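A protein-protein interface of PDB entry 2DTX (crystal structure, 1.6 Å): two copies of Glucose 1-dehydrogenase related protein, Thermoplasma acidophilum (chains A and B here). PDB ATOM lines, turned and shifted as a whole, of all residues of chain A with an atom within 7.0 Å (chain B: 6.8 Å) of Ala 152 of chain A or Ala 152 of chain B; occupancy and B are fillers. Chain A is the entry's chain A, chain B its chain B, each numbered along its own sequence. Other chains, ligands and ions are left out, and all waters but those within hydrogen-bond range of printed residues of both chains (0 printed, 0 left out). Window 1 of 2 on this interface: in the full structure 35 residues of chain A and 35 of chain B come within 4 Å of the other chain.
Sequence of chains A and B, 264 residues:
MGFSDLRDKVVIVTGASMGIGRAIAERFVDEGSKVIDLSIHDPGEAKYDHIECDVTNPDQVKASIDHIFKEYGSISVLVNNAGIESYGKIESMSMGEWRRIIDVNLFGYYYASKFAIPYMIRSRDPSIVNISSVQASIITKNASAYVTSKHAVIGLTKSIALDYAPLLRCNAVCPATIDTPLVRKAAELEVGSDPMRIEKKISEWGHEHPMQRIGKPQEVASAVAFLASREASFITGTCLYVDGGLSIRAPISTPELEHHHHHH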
ATOM      1  N   TRP A  98      19.403 -22.998   0.703  1.00  0.00           N
ATOM      2  CA  TRP A  98      18.706 -23.372  -0.540  1.00  0.00           C
ATOM      3  C   TRP A  98      19.460 -22.716  -1.703  1.00  0.00           C
ATOM      4  O   TRP A  98      19.784 -23.368  -2.718  1.00  0.00           O
ATOM      5  CB  TRP A  98      17.246 -22.861  -0.491  1.00  0.00           C
ATOM      6  CG  TRP A  98      16.296 -23.580  -1.409  1.00  0.00           C
ATOM      7  CD1 TRP A  98      15.528 -24.660  -1.093  1.00  0.00           C
ATOM      8  CD2 TRP A  98      16.024 -23.279  -2.793  1.00  0.00           C
ATOM      9  NE1 TRP A  98      14.793 -25.058  -2.193  1.00  0.00           N
ATOM     10  CE2 TRP A  98      15.078 -24.231  -3.247  1.00  0.00           C
ATOM     11  CE3 TRP A  98      16.486 -22.301  -3.689  1.00  0.00           C
ATOM     12  CZ2 TRP A  98      14.580 -24.233  -4.564  1.00  0.00           C
ATOM     13  CZ3 TRP A  98      15.990 -22.303  -5.003  1.00  0.00           C
ATOM     14  CH2 TRP A  98      15.048 -23.267  -5.422  1.00  0.00           C
ATOM     15  N   ILE A 102      21.916 -24.150  -5.085  1.00  0.00           N
ATOM     16  CA  ILE A 102      21.774 -23.717  -6.480  1.00  0.00           C
ATOM     17  C   ILE A 102      23.121 -23.120  -6.946  1.00  0.00           C
ATOM     18  O   ILE A 102      23.549 -23.305  -8.090  1.00  0.00           O
ATOM     19  CB  ILE A 102      20.690 -22.627  -6.618  1.00  0.00           C
ATOM     20  CG1 ILE A 102      19.345 -23.133  -6.071  1.00  0.00           C
ATOM     21  CG2 ILE A 102      20.568 -22.192  -8.077  1.00  0.00           C
ATOM     22  CD1 ILE A 102      18.824 -24.436  -6.738  1.00  0.00           C
ATOM     23  N   ASN A 105      25.622 -26.288  -7.419  1.00  0.00           N
ATOM     24  CA  ASN A 105      25.115 -27.229  -8.417  1.00  0.00           C
ATOM     25  C   ASN A 105      24.766 -26.688  -9.782  1.00  0.00           C
ATOM     26  O   ASN A 105      24.872 -27.422 -10.771  1.00  0.00           O
ATOM     27  CB  ASN A 105      23.910 -27.977  -7.840  1.00  0.00           C
ATOM     28  CG  ASN A 105      24.290 -28.870  -6.671  1.00  0.00           C
ATOM     29  OD1 ASN A 105      25.436 -28.859  -6.205  1.00  0.00           O
ATOM     30  ND2 ASN A 105      23.328 -29.641  -6.178  1.00  0.00           N
ATOM     31  N   LEU A 106      24.338 -25.427  -9.848  1.00  0.00           N
ATOM     32  CA  LEU A 106      24.010 -24.834 -11.135  1.00  0.00           C
ATOM     33  C   LEU A 106      24.998 -23.742 -11.544  1.00  0.00           C
ATOM     34  O   LEU A 106      25.598 -23.800 -12.620  1.00  0.00           O
ATOM     35  CB  LEU A 106      22.605 -24.244 -11.116  1.00  0.00           C
ATOM     36  CG  LEU A 106      22.266 -23.400 -12.351  1.00  0.00           C
ATOM     37  CD1 LEU A 106      22.275 -24.280 -13.603  1.00  0.00           C
ATOM     38  CD2 LEU A 106      20.912 -22.721 -12.165  1.00  0.00           C
ATOM     39  N   SER A 132      24.347 -34.618 -13.964  1.00  0.00           N
ATOM     40  CA  SER A 132      23.064 -34.230 -13.405  1.00  0.00           C
ATOM     41  C   SER A 132      22.669 -35.311 -12.401  1.00  0.00           C
ATOM     42  O   SER A 132      23.454 -35.603 -11.493  1.00  0.00           O
ATOM     43  CB  SER A 132      22.015 -34.073 -14.518  1.00  0.00           C
ATOM     44  OG  SER A 132      20.771 -33.630 -13.992  1.00  0.00           O
ATOM     45  N   ALA A 136      16.629 -35.675 -12.289  1.00  0.00           N
ATOM     46  CA  ALA A 136      16.204 -34.706 -13.298  1.00  0.00           C
ATOM     47  C   ALA A 136      14.842 -35.255 -13.805  1.00  0.00           C
ATOM     48  O   ALA A 136      14.116 -34.565 -14.528  1.00  0.00           O
ATOM     49  CB  ALA A 136      17.198 -34.642 -14.465  1.00  0.00           C
ATOM     50  N   TYR A 146      18.150 -29.433  -4.259  1.00  0.00           N
ATOM     51  CA  TYR A 146      18.952 -30.364  -5.026  1.00  0.00           C
ATOM     52  C   TYR A 146      18.210 -30.739  -6.311  1.00  0.00           C
ATOM     53  O   TYR A 146      18.768 -30.673  -7.408  1.00  0.00           O
ATOM     54  CB  TYR A 146      19.218 -31.619  -4.203  1.00  0.00           C
ATOM     55  CG  TYR A 146      19.996 -32.677  -4.942  1.00  0.00           C
ATOM     56  CD1 TYR A 146      21.395 -32.661  -4.979  1.00  0.00           C
ATOM     57  CD2 TYR A 146      19.335 -33.713  -5.601  1.00  0.00           C
ATOM     58  CE1 TYR A 146      22.105 -33.661  -5.649  1.00  0.00           C
ATOM     59  CE2 TYR A 146      20.028 -34.706  -6.267  1.00  0.00           C
ATOM     60  CZ  TYR A 146      21.406 -34.683  -6.289  1.00  0.00           C
ATOM     61  OH  TYR A 146      22.095 -35.685  -6.937  1.00  0.00           O
ATOM     62  N   VAL A 147      16.947 -31.130  -6.163  1.00  0.00           N
ATOM     63  CA  VAL A 147      16.145 -31.528  -7.313  1.00  0.00           C
ATOM     64  C   VAL A 147      16.025 -30.371  -8.316  1.00  0.00           C
ATOM     65  O   VAL A 147      16.168 -30.561  -9.535  1.00  0.00           O
ATOM     66  CB  VAL A 147      14.754 -31.993  -6.839  1.00  0.00           C
ATOM     67  CG1 VAL A 147      13.802 -32.119  -8.016  1.00  0.00           C
ATOM     68  CG2 VAL A 147      14.900 -33.341  -6.116  1.00  0.00           C
ATOM     69  N   THR A 148      15.786 -29.168  -7.810  1.00  0.00           N
ATOM     70  CA  THR A 148      15.667 -28.002  -8.685  1.00  0.00           C
ATOM     71  C   THR A 148      16.983 -27.793  -9.448  1.00  0.00           C
ATOM     72  O   THR A 148      16.989 -27.556 -10.660  1.00  0.00           O
ATOM     73  CB  THR A 148      15.339 -26.742  -7.858  1.00  0.00           C
ATOM     74  OG1 THR A 148      14.055 -26.919  -7.245  1.00  0.00           O
ATOM     75  CG2 THR A 148      15.277 -25.503  -8.747  1.00  0.00           C
ATOM     76  N   SER A 149      18.101 -27.881  -8.741  1.00  0.00           N
ATOM     77  CA  SER A 149      19.382 -27.676  -9.402  1.00  0.00           C
ATOM     78  C   SER A 149      19.679 -28.704 -10.479  1.00  0.00           C
ATOM     79  O   SER A 149      20.268 -28.361 -11.509  1.00  0.00           O
ATOM     80  CB  SER A 149      20.522 -27.642  -8.365  1.00  0.00           C
ATOM     81  OG  SER A 149      20.849 -28.928  -7.849  1.00  0.00           O
ATOM     82  N   LYS A 150      19.260 -29.949 -10.271  1.00  0.00           N
ATOM     83  CA  LYS A 150      19.559 -30.978 -11.263  1.00  0.00           C
ATOM     84  C   LYS A 150      18.719 -30.842 -12.521  1.00  0.00           C
ATOM     85  O   LYS A 150      19.194 -31.171 -13.616  1.00  0.00           O
ATOM     86  CB  LYS A 150      19.454 -32.371 -10.639  1.00  0.00           C
ATOM     87  CG  LYS A 150      20.535 -32.629  -9.554  1.00  0.00           C
ATOM     88  CD  LYS A 150      21.922 -32.432 -10.161  1.00  0.00           C
ATOM     89  CE  LYS A 150      23.052 -32.900  -9.257  1.00  0.00           C
ATOM     90  NZ  LYS A 150      24.355 -32.893 -10.002  1.00  0.00           N
ATOM     91  N   HIS A 151      17.489 -30.350 -12.364  1.00  0.00           N
ATOM     92  CA  HIS A 151      16.639 -30.057 -13.517  1.00  0.00           C
ATOM     93  C   HIS A 151      17.281 -28.876 -14.267  1.00  0.00           C
ATOM     94  O   HIS A 151      17.355 -28.873 -15.490  1.00  0.00           O
ATOM     95  CB  HIS A 151      15.215 -29.673 -13.060  1.00  0.00           C
ATOM     96  CG  HIS A 151      14.332 -30.851 -12.761  1.00  0.00           C
ATOM     97  ND1 HIS A 151      14.529 -31.687 -11.679  1.00  0.00           N
ATOM     98  CD2 HIS A 151      13.248 -31.330 -13.418  1.00  0.00           C
ATOM     99  CE1 HIS A 151      13.602 -32.631 -11.688  1.00  0.00           C
ATOM    100  NE2 HIS A 151      12.814 -32.440 -12.732  1.00  0.00           N
ATOM    101  N   ALA A 152      17.755 -27.875 -13.522  1.00  0.00           N
ATOM    102  CA  ALA A 152      18.382 -26.709 -14.139  1.00  0.00           C
ATOM    103  C   ALA A 152      19.578 -27.127 -14.976  1.00  0.00           C
ATOM    104  O   ALA A 152      19.788 -26.600 -16.066  1.00  0.00           O
ATOM    105  CB  ALA A 152      18.821 -25.714 -13.060  1.00  0.00           C
ATOM    106  N   VAL A 153      20.366 -28.070 -14.457  1.00  0.00           N
ATOM    107  CA  VAL A 153      21.542 -28.554 -15.184  1.00  0.00           C
ATOM    108  C   VAL A 153      21.152 -29.114 -16.548  1.00  0.00           C
ATOM    109  O   VAL A 153      21.875 -28.918 -17.521  1.00  0.00           O
ATOM    110  CB  VAL A 153      22.301 -29.630 -14.362  1.00  0.00           C
ATOM    111  CG1 VAL A 153      23.322 -30.370 -15.235  1.00  0.00           C
ATOM    112  CG2 VAL A 153      23.024 -28.953 -13.193  1.00  0.00           C
ATOM    113  N   ILE A 154      20.025 -29.816 -16.627  1.00  0.00           N
ATOM    114  CA  ILE A 154      19.590 -30.333 -17.922  1.00  0.00           C
ATOM    115  C   ILE A 154      19.300 -29.163 -18.880  1.00  0.00           C
ATOM    116  O   ILE A 154      19.655 -29.220 -20.056  1.00  0.00           O
ATOM    117  CB  ILE A 154      18.327 -31.212 -17.767  1.00  0.00           C
ATOM    118  CG1 ILE A 154      18.645 -32.440 -16.910  1.00  0.00           C
ATOM    119  CG2 ILE A 154      17.805 -31.624 -19.156  1.00  0.00           C
ATOM    120  CD1 ILE A 154      19.801 -33.300 -17.462  1.00  0.00           C
ATOM    121  N   GLY A 155      18.662 -28.097 -18.382  1.00  0.00           N
ATOM    122  CA  GLY A 155      18.386 -26.959 -19.249  1.00  0.00           C
ATOM    123  C   GLY A 155      19.667 -26.296 -19.729  1.00  0.00           C
ATOM    124  O   GLY A 155      19.789 -25.930 -20.896  1.00  0.00           O
ATOM    125  N   LEU A 156      20.627 -26.151 -18.828  1.00  0.00           N
ATOM    126  CA  LEU A 156      21.906 -25.541 -19.194  1.00  0.00           C
ATOM    127  C   LEU A 156      22.604 -26.394 -20.244  1.00  0.00           C
ATOM    128  O   LEU A 156      23.192 -25.859 -21.209  1.00  0.00           O
ATOM    129  CB  LEU A 156      22.788 -25.392 -17.951  1.00  0.00           C
ATOM    130  CG  LEU A 156      24.186 -24.822 -18.207  1.00  0.00           C
ATOM    131  CD1 LEU A 156      24.083 -23.364 -18.651  1.00  0.00           C
ATOM    132  CD2 LEU A 156      25.021 -24.951 -16.931  1.00  0.00           C
ATOM    133  N   THR A 157      22.520 -27.708 -20.067  1.00  0.00           N
ATOM    134  CA  THR A 157      23.136 -28.654 -20.997  1.00  0.00           C
ATOM    135  C   THR A 157      22.547 -28.505 -22.391  1.00  0.00           C
ATOM    136  O   THR A 157      23.279 -28.414 -23.366  1.00  0.00           O
ATOM    137  CB  THR A 157      22.927 -30.106 -20.502  1.00  0.00           C
ATOM    138  OG1 THR A 157      23.588 -30.277 -19.243  1.00  0.00           O
ATOM    139  CG2 THR A 157      23.490 -31.126 -21.515  1.00  0.00           C
ATOM    140  N   LYS A 158      21.216 -28.473 -22.491  1.00  0.00           N
ATOM    141  CA  LYS A 158      20.566 -28.339 -23.797  1.00  0.00           C
ATOM    142  C   LYS A 158      20.947 -27.033 -24.457  1.00  0.00           C
ATOM    143  O   LYS A 158      21.195 -26.996 -25.661  1.00  0.00           O
ATOM    144  CB  LYS A 158      19.040 -28.389 -23.657  1.00  0.00           C
ATOM    145  CG  LYS A 158      18.479 -29.746 -23.213  1.00  0.00           C
ATOM    146  CD  LYS A 158      16.958 -29.668 -23.193  1.00  0.00           C
ATOM    147  CE  LYS A 158      16.336 -30.942 -22.650  1.00  0.00           C
ATOM    148  NZ  LYS A 158      14.893 -30.692 -22.318  1.00  0.00           N
ATOM    149  N   ILE B 102      17.580 -15.872 -13.643  1.00  0.00           N
ATOM    150  CA  ILE B 102      17.360 -16.986 -12.714  1.00  0.00           C
ATOM    151  C   ILE B 102      16.633 -16.455 -11.468  1.00  0.00           C
ATOM    152  O   ILE B 102      15.725 -17.106 -10.943  1.00  0.00           O
ATOM    153  CB  ILE B 102      18.683 -17.658 -12.267  1.00  0.00           C
ATOM    154  CG1 ILE B 102      19.470 -18.171 -13.486  1.00  0.00           C
ATOM    155  CG2 ILE B 102      18.381 -18.793 -11.325  1.00  0.00           C
ATOM    156  CD1 ILE B 102      18.703 -19.147 -14.373  1.00  0.00           C
ATOM    157  N   ASN B 105      12.774 -15.661 -12.648  1.00  0.00           N
ATOM    158  CA  ASN B 105      12.066 -16.851 -13.122  1.00  0.00           C
ATOM    159  C   ASN B 105      12.055 -18.061 -12.200  1.00  0.00           C
ATOM    160  O   ASN B 105      11.134 -18.895 -12.294  1.00  0.00           O
ATOM    161  CB  ASN B 105      12.607 -17.270 -14.507  1.00  0.00           C
ATOM    162  CG  ASN B 105      12.323 -16.225 -15.598  1.00  0.00           C
ATOM    163  OD1 ASN B 105      11.741 -15.178 -15.331  1.00  0.00           O
ATOM    164  ND2 ASN B 105      12.731 -16.517 -16.829  1.00  0.00           N
ATOM    165  N   LEU B 106      13.070 -18.182 -11.350  1.00  0.00           N
ATOM    166  CA  LEU B 106      13.144 -19.296 -10.408  1.00  0.00           C
ATOM    167  C   LEU B 106      12.995 -18.851  -8.974  1.00  0.00           C
ATOM    168  O   LEU B 106      12.101 -19.321  -8.280  1.00  0.00           O
ATOM    169  CB  LEU B 106      14.462 -20.085 -10.527  1.00  0.00           C
ATOM    170  CG  LEU B 106      14.689 -21.158  -9.449  1.00  0.00           C
ATOM    171  CD1 LEU B 106      13.575 -22.244  -9.553  1.00  0.00           C
ATOM    172  CD2 LEU B 106      16.098 -21.771  -9.585  1.00  0.00           C
ATOM    173  N   SER B 132       5.716 -22.621 -16.533  1.00  0.00           N
ATOM    174  CA  SER B 132       7.043 -22.942 -17.050  1.00  0.00           C
ATOM    175  C   SER B 132       7.052 -22.560 -18.531  1.00  0.00           C
ATOM    176  O   SER B 132       6.754 -21.416 -18.871  1.00  0.00           O
ATOM    177  CB  SER B 132       7.348 -24.434 -16.841  1.00  0.00           C
ATOM    178  OG  SER B 132       8.652 -24.749 -17.313  1.00  0.00           O
ATOM    179  N   TYR B 146      17.182 -18.275 -19.706  1.00  0.00           N
ATOM    180  CA  TYR B 146      15.745 -18.494 -19.752  1.00  0.00           C
ATOM    181  C   TYR B 146      15.443 -19.987 -19.748  1.00  0.00           C
ATOM    182  O   TYR B 146      14.621 -20.460 -18.963  1.00  0.00           O
ATOM    183  CB  TYR B 146      15.163 -17.872 -21.013  1.00  0.00           C
ATOM    184  CG  TYR B 146      13.671 -18.098 -21.157  1.00  0.00           C
ATOM    185  CD1 TYR B 146      12.753 -17.254 -20.528  1.00  0.00           C
ATOM    186  CD2 TYR B 146      13.182 -19.156 -21.927  1.00  0.00           C
ATOM    187  CE1 TYR B 146      11.385 -17.457 -20.665  1.00  0.00           C
ATOM    188  CE2 TYR B 146      11.812 -19.369 -22.072  1.00  0.00           C
ATOM    189  CZ  TYR B 146      10.926 -18.515 -21.439  1.00  0.00           C
ATOM    190  OH  TYR B 146       9.578 -18.705 -21.585  1.00  0.00           O
ATOM    191  N   VAL B 147      16.105 -20.724 -20.629  1.00  0.00           N
ATOM    192  CA  VAL B 147      15.881 -22.165 -20.721  1.00  0.00           C
ATOM    193  C   VAL B 147      16.211 -22.872 -19.407  1.00  0.00           C
ATOM    194  O   VAL B 147      15.462 -23.744 -18.943  1.00  0.00           O
ATOM    195  CB  VAL B 147      16.713 -22.755 -21.882  1.00  0.00           C
ATOM    196  CG1 VAL B 147      16.678 -24.250 -21.848  1.00  0.00           C
ATOM    197  CG2 VAL B 147      16.160 -22.241 -23.224  1.00  0.00           C
ATOM    198  N   THR B 148      17.322 -22.490 -18.792  1.00  0.00           N
ATOM    199  CA  THR B 148      17.724 -23.092 -17.540  1.00  0.00           C
ATOM    200  C   THR B 148      16.653 -22.823 -16.482  1.00  0.00           C
ATOM    201  O   THR B 148      16.254 -23.730 -15.742  1.00  0.00           O
ATOM    202  CB  THR B 148      19.087 -22.508 -17.099  1.00  0.00           C
ATOM    203  OG1 THR B 148      20.077 -22.870 -18.067  1.00  0.00           O
ATOM    204  CG2 THR B 148      19.499 -23.033 -15.748  1.00  0.00           C
ATOM    205  N   SER B 149      16.192 -21.575 -16.405  1.00  0.00           N
ATOM    206  CA  SER B 149      15.191 -21.232 -15.407  1.00  0.00           C
ATOM    207  C   SER B 149      13.898 -22.017 -15.577  1.00  0.00           C
ATOM    208  O   SER B 149      13.296 -22.427 -14.580  1.00  0.00           O
ATOM    209  CB  SER B 149      14.890 -19.720 -15.416  1.00  0.00           C
ATOM    210  OG  SER B 149      14.124 -19.299 -16.536  1.00  0.00           O
ATOM    211  N   LYS B 150      13.493 -22.264 -16.823  1.00  0.00           N
ATOM    212  CA  LYS B 150      12.235 -22.973 -17.053  1.00  0.00           C
ATOM    213  C   LYS B 150      12.354 -24.450 -16.700  1.00  0.00           C
ATOM    214  O   LYS B 150      11.385 -25.052 -16.239  1.00  0.00           O
ATOM    215  CB  LYS B 150      11.767 -22.754 -18.493  1.00  0.00           C
ATOM    216  CG  LYS B 150      11.313 -21.287 -18.760  1.00  0.00           C
ATOM    217  CD  LYS B 150      10.203 -20.856 -17.779  1.00  0.00           C
ATOM    218  CE  LYS B 150       9.549 -19.511 -18.114  1.00  0.00           C
ATOM    219  NZ  LYS B 150       8.385 -19.205 -17.176  1.00  0.00           N
ATOM    220  N   HIS B 151      13.530 -25.036 -16.925  1.00  0.00           N
ATOM    221  CA  HIS B 151      13.766 -26.416 -16.512  1.00  0.00           C
ATOM    222  C   HIS B 151      13.769 -26.436 -14.977  1.00  0.00           C
ATOM    223  O   HIS B 151      13.224 -27.353 -14.347  1.00  0.00           O
ATOM    224  CB  HIS B 151      15.132 -26.927 -17.002  1.00  0.00           C
ATOM    225  CG  HIS B 151      15.138 -27.404 -18.423  1.00  0.00           C
ATOM    226  ND1 HIS B 151      14.993 -26.558 -19.502  1.00  0.00           N
ATOM    227  CD2 HIS B 151      15.276 -28.652 -18.935  1.00  0.00           C
ATOM    228  CE1 HIS B 151      15.048 -27.267 -20.620  1.00  0.00           C
ATOM    229  NE2 HIS B 151      15.219 -28.539 -20.306  1.00  0.00           N
ATOM    230  N   ALA B 152      14.388 -25.430 -14.366  1.00  0.00           N
ATOM    231  CA  ALA B 152      14.440 -25.359 -12.902  1.00  0.00           C
ATOM    232  C   ALA B 152      13.026 -25.323 -12.310  1.00  0.00           C
ATOM    233  O   ALA B 152      12.765 -25.952 -11.283  1.00  0.00           O
ATOM    234  CB  ALA B 152      15.225 -24.111 -12.458  1.00  0.00           C
ATOM    235  N   VAL B 153      12.132 -24.580 -12.952  1.00  0.00           N
ATOM    236  CA  VAL B 153      10.752 -24.490 -12.476  1.00  0.00           C
ATOM    237  C   VAL B 153      10.112 -25.871 -12.422  1.00  0.00           C
ATOM    238  O   VAL B 153       9.319 -26.144 -11.528  1.00  0.00           O
ATOM    239  CB  VAL B 153       9.906 -23.576 -13.375  1.00  0.00           C
ATOM    240  CG1 VAL B 153       8.414 -23.738 -13.042  1.00  0.00           C
ATOM    241  CG2 VAL B 153      10.325 -22.109 -13.142  1.00  0.00           C
ATOM    242  N   ILE B 154      10.431 -26.731 -13.382  1.00  0.00           N
ATOM    243  CA  ILE B 154       9.861 -28.080 -13.358  1.00  0.00           C
ATOM    244  C   ILE B 154      10.348 -28.838 -12.122  1.00  0.00           C
ATOM    245  O   ILE B 154       9.569 -29.526 -11.441  1.00  0.00           O
ATOM    246  CB  ILE B 154      10.219 -28.849 -14.646  1.00  0.00           C
ATOM    247  CG1 ILE B 154       9.616 -28.134 -15.865  1.00  0.00           C
ATOM    248  CG2 ILE B 154       9.726 -30.312 -14.539  1.00  0.00           C
ATOM    249  CD1 ILE B 154       8.118 -27.884 -15.782  1.00  0.00           C
ATOM    250  N   GLY B 155      11.632 -28.714 -11.803  1.00  0.00           N
ATOM    251  CA  GLY B 155      12.140 -29.400 -10.627  1.00  0.00           C
ATOM    252  C   GLY B 155      11.482 -28.872  -9.354  1.00  0.00           C
ATOM    253  O   GLY B 155      11.144 -29.643  -8.450  1.00  0.00           O
ATOM    254  N   LEU B 156      11.299 -27.558  -9.281  1.00  0.00           N
ATOM    255  CA  LEU B 156      10.680 -26.943  -8.105  1.00  0.00           C
ATOM    256  C   LEU B 156       9.255 -27.462  -7.958  1.00  0.00           C
ATOM    257  O   LEU B 156       8.785 -27.759  -6.859  1.00  0.00           O
ATOM    258  CB  LEU B 156      10.657 -25.420  -8.243  1.00  0.00           C
ATOM    259  CG  LEU B 156      10.023 -24.698  -7.041  1.00  0.00           C
ATOM    260  CD1 LEU B 156      10.825 -24.927  -5.742  1.00  0.00           C
ATOM    261  CD2 LEU B 156       9.970 -23.207  -7.372  1.00  0.00           C
ATOM    262  N   THR B 157       8.576 -27.574  -9.086  1.00  0.00           N
ATOM    263  CA  THR B 157       7.197 -28.055  -9.125  1.00  0.00           C
ATOM    264  C   THR B 157       7.080 -29.481  -8.610  1.00  0.00           C
ATOM    265  O   THR B 157       6.225 -29.772  -7.771  1.00  0.00           O
ATOM    266  CB  THR B 157       6.679 -28.009 -10.564  1.00  0.00           C
ATOM    267  OG1 THR B 157       6.650 -26.653 -11.012  1.00  0.00           O
ATOM    268  CG2 THR B 157       5.270 -28.595 -10.660  1.00  0.00           C
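Printed residues of chain B within 4 Å of Leu 106 of chain A: Thr 148.
Of the printed residues of chain B, Ala 152 of chain A touches Thr 148 and Ala 152.
Of the printed residues of chain B, Gly 155 of chain A touches Val 147, Thr 148 and His 151.
Ile 102 of chain B touches none of the printed residues of chain A.
Ser 132 of chain B touches none of the printed residues of chain A.
Of the printed residues of chain A, Val 147 of chain B touches Gly 155 (3.7 Å).
Printed residues of chain A within 4 Å of His 151 of chain B: His 151 (3.3 Å), Ile 154 (3.9 Å), Gly 155 (3.4 Å) and Lys 158 (3.0 Å).
Printed residues of chain A within 4 Å of Ala 152 of chain B: Thr 148 (3.6 Å) and Ala 152 (3.98 Å).
Printed residues of chain A within 4 Å of Leu 156 of chain B: Trp 98 (3.996 Å) and Thr 148 (3.5 Å).
The nearest printed residue of chain A that does not touch Leu 106 of chain B is Trp 98 of chain A (4.5 Å).
Printed residues of chain A that touch a printed residue of chain B: Trp 98, Leu 106, Val 147, Thr 148, His 151, Ala 152, Ile 154, Gly 155, Leu 156 and Lys 158.
Printed residues of chain B that touch a printed residue of chain A: Leu 106, Val 147, Thr 148, His 151, Ala 152, Ile 154, Gly 155 and Leu 156.
Hydrophobic or aromatic side chains of chain B that line the printed part of chain A: Leu 106, Val 147, His 151, Ala 152, Ile 154 and Leu 156.
Among the printed residues, 18 pairs touch across the chains.
Among the printed residues, no Asp or Glu carboxylate lies within 4 Å of a Lys or Arg side-chain nitrogen of the other chain.
The backbone carbonyl oxygen (O) of Val 147 of chain B lies within hydrogen-bond range of a ring nitrogen (ND1) of His 151 of chain B (2.9 Å).
O of Ala 136 of chain A lies within hydrogen-bond range of NE2 of His 151 of chain A (3.1 Å).
A ring nitrogen (ND1) of His 151 of chain A lies within hydrogen-bond range of the backbone carbonyl oxygen (O) of Val 147 of chain A, 2.9 Å away.
Among the printed residues, merely in contact across the chains: His 151 of chain A with His 151 of chain B (3.3 Å), Gly 155 of chain A with His 151 of chain B (3.4 Å), His 151 of chain A with Gly 155 of chain B (3.4 Å), Ala 152 of chain A with Thr 148 of chain B (3.6 Å), Thr 148 of chain A with Ala 152 of chain B (3.6 Å), Val 147 of chain A with Gly 155 of chain B (3.7 Å), Gly 155 of chain A with Val 147 of chain B (3.7 Å), Leu 106 of chain A with Thr 148 of chain B (3.7 Å), Thr 148 of chain A with Leu 106 of chain B (3.8 Å), Gly 155 of chain A with Thr 148 of chain B (3.8 Å), His 151 of chain A with Ile 154 of chain B (3.8 Å), Thr 148 of chain A with Gly 155 of chain B (3.9 Å), Ile 154 of chain A with His 151 of chain B (3.9 Å), Ala 152 of chain A with Ala 152 of chain B (3.98 Å) and Trp 98 of chain A with Leu 156 of chain B (3.996 Å).
The side-chain hydroxyl (OG1) of Thr 148 of chain A lies close to the backbone NH (N) of Leu 156 of chain B, at 3.5 Å.
The side-chain hydroxyl (OG1) of Thr 148 of chain B lies within hydrogen-bond range of the backbone NH (N) of Leu 156 of chain A, 3.4 Å away.
A ring nitrogen (NE2) of His 151 of chain B sits at hydrogen-bond distance from the side-chain amino group (NZ) of Lys 158 of chain A.
Leu 106 of chain A touches Thr 148 of chain B, and with the chains exchanged Thr 148 of chain A touches Leu 106 of chain B.
Thr 148 of chain A touches Leu 156 of chain B, and with the chains exchanged Leu 156 of chain A touches Thr 148 of chain B.
His 151 of chain A touches its own counterpart, His 151 of chain B.
His 151 of chain A touches Ile 154 of chain B, and with the chains exchanged Ile 154 of chain A touches His 151 of chain B.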
